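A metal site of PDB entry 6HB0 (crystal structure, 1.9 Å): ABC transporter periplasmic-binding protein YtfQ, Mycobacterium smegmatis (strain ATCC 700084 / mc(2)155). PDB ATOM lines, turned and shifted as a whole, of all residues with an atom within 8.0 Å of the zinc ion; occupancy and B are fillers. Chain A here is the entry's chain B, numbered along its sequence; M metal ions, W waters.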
ATOM      1  N   GLY A 123       4.040   8.642 -18.357  1.00  0.00           N
ATOM      2  CA  GLY A 123       4.985   8.997 -19.420  1.00  0.00           C
ATOM      3  C   GLY A 123       5.350  10.467 -19.318  1.00  0.00           C
ATOM      4  O   GLY A 123       4.862  11.182 -18.427  1.00  0.00           O
ATOM      5  N   ALA A 124       6.260  10.891 -20.189  1.00  0.00           N
ATOM      6  CA  ALA A 124       6.716  12.263 -20.163  1.00  0.00           C
ATOM      7  C   ALA A 124       5.580  13.110 -20.711  1.00  0.00           C
ATOM      8  O   ALA A 124       4.854  12.676 -21.580  1.00  0.00           O
ATOM      9  CB  ALA A 124       7.961  12.426 -20.992  1.00  0.00           C
ATOM     10  N   ASP A 125       5.479  14.303 -20.185  1.00  0.00           N
ATOM     11  CA  ASP A 125       4.613  15.376 -20.676  1.00  0.00           C
ATOM     12  C   ASP A 125       5.412  16.363 -21.571  1.00  0.00           C
ATOM     13  O   ASP A 125       6.094  17.233 -21.075  1.00  0.00           O
ATOM     14  CB  ASP A 125       4.097  16.114 -19.471  1.00  0.00           C
ATOM     15  CG  ASP A 125       3.024  17.169 -19.820  1.00  0.00           C
ATOM     16  OD1 ASP A 125       2.837  17.529 -21.026  1.00  0.00           O
ATOM     17  OD2 ASP A 125       2.379  17.593 -18.845  1.00  0.00           O
ATOM     18  N   PHE A 126       5.316  16.183 -22.873  1.00  0.00           N
ATOM     19  CA  PHE A 126       6.116  16.910 -23.816  1.00  0.00           C
ATOM     20  C   PHE A 126       5.642  18.377 -23.924  1.00  0.00           C
ATOM     21  O   PHE A 126       6.440  19.233 -24.180  1.00  0.00           O
ATOM     22  CB  PHE A 126       6.009  16.259 -25.181  1.00  0.00           C
ATOM     23  CG  PHE A 126       6.409  14.810 -25.198  1.00  0.00           C
ATOM     24  CD1 PHE A 126       7.631  14.417 -24.710  1.00  0.00           C
ATOM     25  CD2 PHE A 126       5.536  13.832 -25.723  1.00  0.00           C
ATOM     26  CE1 PHE A 126       8.016  13.078 -24.735  1.00  0.00           C
ATOM     27  CE2 PHE A 126       5.896  12.479 -25.717  1.00  0.00           C
ATOM     28  CZ  PHE A 126       7.136  12.118 -25.227  1.00  0.00           C
ATOM     29  N   ILE A 127       4.360  18.642 -23.725  1.00  0.00           N
ATOM     30  CA  ILE A 127       3.860  20.048 -23.683  1.00  0.00           C
ATOM     31  C   ILE A 127       4.534  20.758 -22.555  1.00  0.00           C
ATOM     32  O   ILE A 127       5.074  21.845 -22.716  1.00  0.00           O
ATOM     33  CB  ILE A 127       2.335  20.140 -23.534  1.00  0.00           C
ATOM     34  CG1 ILE A 127       1.681  19.508 -24.757  1.00  0.00           C
ATOM     35  CG2 ILE A 127       1.927  21.598 -23.306  1.00  0.00           C
ATOM     36  CD1 ILE A 127       0.167  19.694 -24.885  1.00  0.00           C
ATOM     37  N   GLU A 128       4.568  20.134 -21.406  1.00  0.00           N
ATOM     38  CA  GLU A 128       5.181  20.724 -20.230  1.00  0.00           C
ATOM     39  C   GLU A 128       6.659  20.984 -20.471  1.00  0.00           C
ATOM     40  O   GLU A 128       7.192  21.993 -20.036  1.00  0.00           O
ATOM     41  CB  GLU A 128       4.989  19.794 -19.034  1.00  0.00           C
ATOM     42  CG  GLU A 128       5.642  20.203 -17.754  1.00  0.00           C
ATOM     43  CD  GLU A 128       6.561  19.095 -17.274  1.00  0.00           C
ATOM     44  OE1 GLU A 128       6.097  18.229 -16.524  1.00  0.00           O
ATOM     45  OE2 GLU A 128       7.748  19.081 -17.654  1.00  0.00           O
ATOM     46  N   GLU A 129       7.352  20.091 -21.186  1.00  0.00           N
ATOM     47  CA  GLU A 129       8.785  20.350 -21.516  1.00  0.00           C
ATOM     48  C   GLU A 129       8.936  21.619 -22.307  1.00  0.00           C
ATOM     49  O   GLU A 129       9.772  22.443 -21.996  1.00  0.00           O
ATOM     50  CB  GLU A 129       9.427  19.216 -22.359  1.00  0.00           C
ATOM     51  CG  GLU A 129       9.693  17.969 -21.570  1.00  0.00           C
ATOM     52  CD  GLU A 129      10.297  16.809 -22.378  1.00  0.00           C
ATOM     53  OE1 GLU A 129       9.805  16.570 -23.493  1.00  0.00           O
ATOM     54  OE2 GLU A 129      11.230  16.103 -21.852  1.00  0.00           O
ATOM     55  N   ARG A 131       6.822  24.045 -22.543  1.00  0.00           N
ATOM     56  CA  ARG A 131       6.464  25.167 -21.703  1.00  0.00           C
ATOM     57  C   ARG A 131       7.556  25.626 -20.782  1.00  0.00           C
ATOM     58  O   ARG A 131       7.781  26.827 -20.608  1.00  0.00           O
ATOM     59  CB  ARG A 131       5.208  24.842 -20.874  1.00  0.00           C
ATOM     60  CG  ARG A 131       4.677  26.041 -20.104  1.00  0.00           C
ATOM     61  CD  ARG A 131       3.250  25.796 -19.656  1.00  0.00           C
ATOM     62  NE  ARG A 131       3.298  24.732 -18.734  1.00  0.00           N
ATOM     63  CZ  ARG A 131       2.635  23.591 -18.764  1.00  0.00           C
ATOM     64  NH1 ARG A 131       1.648  23.329 -19.591  1.00  0.00           N
ATOM     65  NH2 ARG A 131       2.957  22.754 -17.816  1.00  0.00           N
ATOM     66  N   ARG A 132       8.236  24.698 -20.146  1.00  0.00           N
ATOM     67  CA  ARG A 132       9.335  25.090 -19.272  1.00  0.00           C
ATOM     68  C   ARG A 132      10.521  25.708 -20.053  1.00  0.00           C
ATOM     69  O   ARG A 132      11.175  26.636 -19.576  1.00  0.00           O
ATOM     70  CB  ARG A 132       9.747  23.904 -18.404  1.00  0.00           C
ATOM     71  CG  ARG A 132       8.651  23.437 -17.428  1.00  0.00           C
ATOM     72  CD  ARG A 132       8.771  21.933 -17.063  1.00  0.00           C
ATOM     73  NE  ARG A 132      10.074  21.758 -16.569  1.00  0.00           N
ATOM     74  CZ  ARG A 132      10.908  20.753 -16.729  1.00  0.00           C
ATOM     75  NH1 ARG A 132      10.588  19.600 -17.294  1.00  0.00           N
ATOM     76  NH2 ARG A 132      12.103  20.940 -16.231  1.00  0.00           N
ATOM     77  N   GLU A 262      14.018  18.575 -19.024  1.00  0.00           N
ATOM     78  CA  GLU A 262      13.544  17.237 -19.393  1.00  0.00           C
ATOM     79  C   GLU A 262      12.408  16.871 -18.507  1.00  0.00           C
ATOM     80  O   GLU A 262      12.427  17.202 -17.363  1.00  0.00           O
ATOM     81  CB  GLU A 262      14.650  16.186 -19.286  1.00  0.00           C
ATOM     82  CG  GLU A 262      14.177  14.844 -19.789  1.00  0.00           C
ATOM     83  CD  GLU A 262      15.227  13.730 -19.761  1.00  0.00           C
ATOM     84  OE1 GLU A 262      16.438  13.989 -19.900  1.00  0.00           O
ATOM     85  OE2 GLU A 262      14.787  12.586 -19.678  1.00  0.00           O
ATOM     86  N   CYS A 263      11.390  16.222 -19.084  1.00  0.00           N
ATOM     87  CA  CYS A 263      10.346  15.579 -18.313  1.00  0.00           C
ATOM     88  C   CYS A 263      10.660  14.107 -18.443  1.00  0.00           C
ATOM     89  O   CYS A 263      10.728  13.572 -19.551  1.00  0.00           O
ATOM     90  CB  CYS A 263       8.972  15.890 -18.886  1.00  0.00           C
ATOM     91  SG  CYS A 263       7.648  15.149 -17.906  1.00  0.00           S
ATOM     92  N   ASN A 264      10.888  13.434 -17.314  1.00  0.00           N
ATOM     93  CA  ASN A 264      11.295  12.018 -17.369  1.00  0.00           C
ATOM     94  C   ASN A 264      10.212  11.070 -17.929  1.00  0.00           C
ATOM     95  O   ASN A 264       9.011  11.296 -17.794  1.00  0.00           O
ATOM     96  CB  ASN A 264      11.631  11.494 -15.969  1.00  0.00           C
ATOM     97  CG  ASN A 264      12.935  12.060 -15.390  1.00  0.00           C
ATOM     98  OD1 ASN A 264      13.132  11.964 -14.198  1.00  0.00           O
ATOM     99  ND2 ASN A 264      13.813  12.619 -16.220  1.00  0.00           N
ATOM    100  N   PRO A 265      10.635   9.996 -18.573  1.00  0.00           N
ATOM    101  CA  PRO A 265       9.707   8.918 -18.820  1.00  0.00           C
ATOM    102  C   PRO A 265       9.357   8.159 -17.519  1.00  0.00           C
ATOM    103  O   PRO A 265       9.795   8.534 -16.429  1.00  0.00           O
ATOM    104  CB  PRO A 265      10.510   8.027 -19.772  1.00  0.00           C
ATOM    105  CG  PRO A 265      11.883   8.140 -19.259  1.00  0.00           C
ATOM    106  CD  PRO A 265      12.018   9.583 -18.837  1.00  0.00           C
ATOM    107  N   ARG A 287      -2.894  10.703 -14.867  1.00  0.00           N
ATOM    108  CA  ARG A 287      -1.555  10.841 -15.392  1.00  0.00           C
ATOM    109  C   ARG A 287      -0.605  10.993 -14.234  1.00  0.00           C
ATOM    110  O   ARG A 287      -0.779  11.853 -13.406  1.00  0.00           O
ATOM    111  CB  ARG A 287      -1.479  12.094 -16.210  1.00  0.00           C
ATOM    112  CG  ARG A 287      -1.592  11.880 -17.693  1.00  0.00           C
ATOM    113  CD  ARG A 287      -0.197  12.096 -18.250  1.00  0.00           C
ATOM    114  NE  ARG A 287      -0.212  12.678 -19.561  1.00  0.00           N
ATOM    115  CZ  ARG A 287       0.885  12.921 -20.244  1.00  0.00           C
ATOM    116  NH1 ARG A 287       0.747  13.464 -21.419  1.00  0.00           N
ATOM    117  NH2 ARG A 287       2.115  12.619 -19.764  1.00  0.00           N
ATOM    118  N   VAL A 288       0.353  10.118 -14.127  1.00  0.00           N
ATOM    119  CA  VAL A 288       1.357  10.283 -13.121  1.00  0.00           C
ATOM    120  C   VAL A 288       2.187  11.463 -13.577  1.00  0.00           C
ATOM    121  O   VAL A 288       2.461  11.617 -14.773  1.00  0.00           O
ATOM    122  CB  VAL A 288       2.205   9.026 -13.051  1.00  0.00           C
ATOM    123  CG1 VAL A 288       3.438   9.253 -12.238  1.00  0.00           C
ATOM    124  CG2 VAL A 288       1.426   7.941 -12.380  1.00  0.00           C
ATOM    125  N   VAL A 289       2.626  12.299 -12.645  1.00  0.00           N
ATOM    126  CA  VAL A 289       3.593  13.308 -13.014  1.00  0.00           C
ATOM    127  C   VAL A 289       4.998  12.762 -12.729  1.00  0.00           C
ATOM    128  O   VAL A 289       5.333  12.501 -11.585  1.00  0.00           O
ATOM    129  CB  VAL A 289       3.336  14.659 -12.316  1.00  0.00           C
ATOM    130  CG1 VAL A 289       1.868  15.106 -12.552  1.00  0.00           C
ATOM    131  CG2 VAL A 289       3.691  14.566 -10.864  1.00  0.00           C
ATOM    132  N   THR A 290       5.789  12.548 -13.779  1.00  0.00           N
ATOM    133  CA  THR A 290       7.140  12.012 -13.632  1.00  0.00           C
ATOM    134  C   THR A 290       8.039  13.135 -13.137  1.00  0.00           C
ATOM    135  O   THR A 290       7.618  14.290 -13.125  1.00  0.00           O
ATOM    136  CB  THR A 290       7.669  11.474 -14.980  1.00  0.00           C
ATOM    137  OG1 THR A 290       7.520  12.472 -16.004  1.00  0.00           O
ATOM    138  CG2 THR A 290       6.874  10.235 -15.378  1.00  0.00           C
ATOM    139  N   PRO A 291       9.235  12.821 -12.676  1.00  0.00           N
ATOM    140  CA  PRO A 291      10.130  13.897 -12.254  1.00  0.00           C
ATOM    141  C   PRO A 291      10.627  14.746 -13.417  1.00  0.00           C
ATOM    142  O   PRO A 291      10.725  14.277 -14.593  1.00  0.00           O
ATOM    143  CB  PRO A 291      11.309  13.150 -11.608  1.00  0.00           C
ATOM    144  CG  PRO A 291      10.740  11.839 -11.247  1.00  0.00           C
ATOM    145  CD  PRO A 291       9.790  11.504 -12.355  1.00  0.00           C
ATOM    146  N   ASP A 292      10.909  15.985 -13.075  1.00  0.00           N
ATOM    147  CA  ASP A 292      11.414  16.964 -14.007  1.00  0.00           C
ATOM    148  C   ASP A 292      12.845  17.324 -13.689  1.00  0.00           C
ATOM    149  O   ASP A 292      13.258  17.353 -12.544  1.00  0.00           O
ATOM    150  CB  ASP A 292      10.512  18.200 -13.949  1.00  0.00           C
ATOM    151  CG  ASP A 292       9.171  17.961 -14.526  1.00  0.00           C
ATOM    152  OD1 ASP A 292       9.021  17.114 -15.448  1.00  0.00           O
ATOM    153  OD2 ASP A 292       8.213  18.599 -14.070  1.00  0.00           O
ATOM    154  N   GLU A 293      13.609  17.550 -14.731  1.00  0.00           N
ATOM    155  CA  GLU A 293      14.997  17.956 -14.643  1.00  0.00           C
ATOM    156  C   GLU A 293      15.147  19.311 -15.336  1.00  0.00           C
ATOM    157  O   GLU A 293      14.418  19.585 -16.306  1.00  0.00           O
ATOM    158  CB  GLU A 293      15.853  16.918 -15.346  1.00  0.00           C
ATOM    159  CG  GLU A 293      15.829  15.565 -14.658  1.00  0.00           C
ATOM    160  CD  GLU A 293      16.788  14.522 -15.253  1.00  0.00           C
ATOM    161  OE1 GLU A 293      17.944  14.855 -15.604  1.00  0.00           O
ATOM    162  OE2 GLU A 293      16.397  13.349 -15.328  1.00  0.00           O
HETATM  163 ZN    ZN M   1       7.343  16.625 -16.343  1.00  0.00          ZN
HETATM  164  O   HOH W   1       6.163  15.836 -14.890  1.00  0.00           O
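The zinc ion is bound by the side-chain carboxylate of Asp 292 (2.0 Å), water W1 (2.0 Å), the side-chain carboxylate of Glu 128 (2.0 Å) and the side-chain sulfur of Cys 263 (2.2 Å). The zinc ion has four donor atoms within binding distance. Slightly farther from the zinc ion lies OE2 of Glu 128 (2.8 Å).
Merely in contact with the zinc ion: Thr 290 (3.99 Å). Of the 20 residues printed, 4 come within 4 Å of the zinc ion.
The side-chain sulfur (SG) of Cys 263 sits close to the side-chain hydroxyl (OG1) of Thr 290 (3.3 Å). The side-chain carboxylate (OE2) of Glu 129 sits at hydrogen-bond distance from the backbone NH (N) of Cys 263 (2.8 Å). SG of Cys 263 sits close to N of Asp 125. The guanidinium group of Arg 132 lies within salt-bridge range of the side-chain carboxylate of Glu 128. The side-chain carboxylate (OD1) of Asp 292 lies close to the guanidinium group (NH1) of Arg 132 (3.5 Å). N of Glu 128 sits at hydrogen-bond distance from OD1 of Asp 125 (3.2 Å). The side-chain hydroxyl of Thr 290 is in hydrogen-bond range of the backbone carbonyl oxygen of Asn 264.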
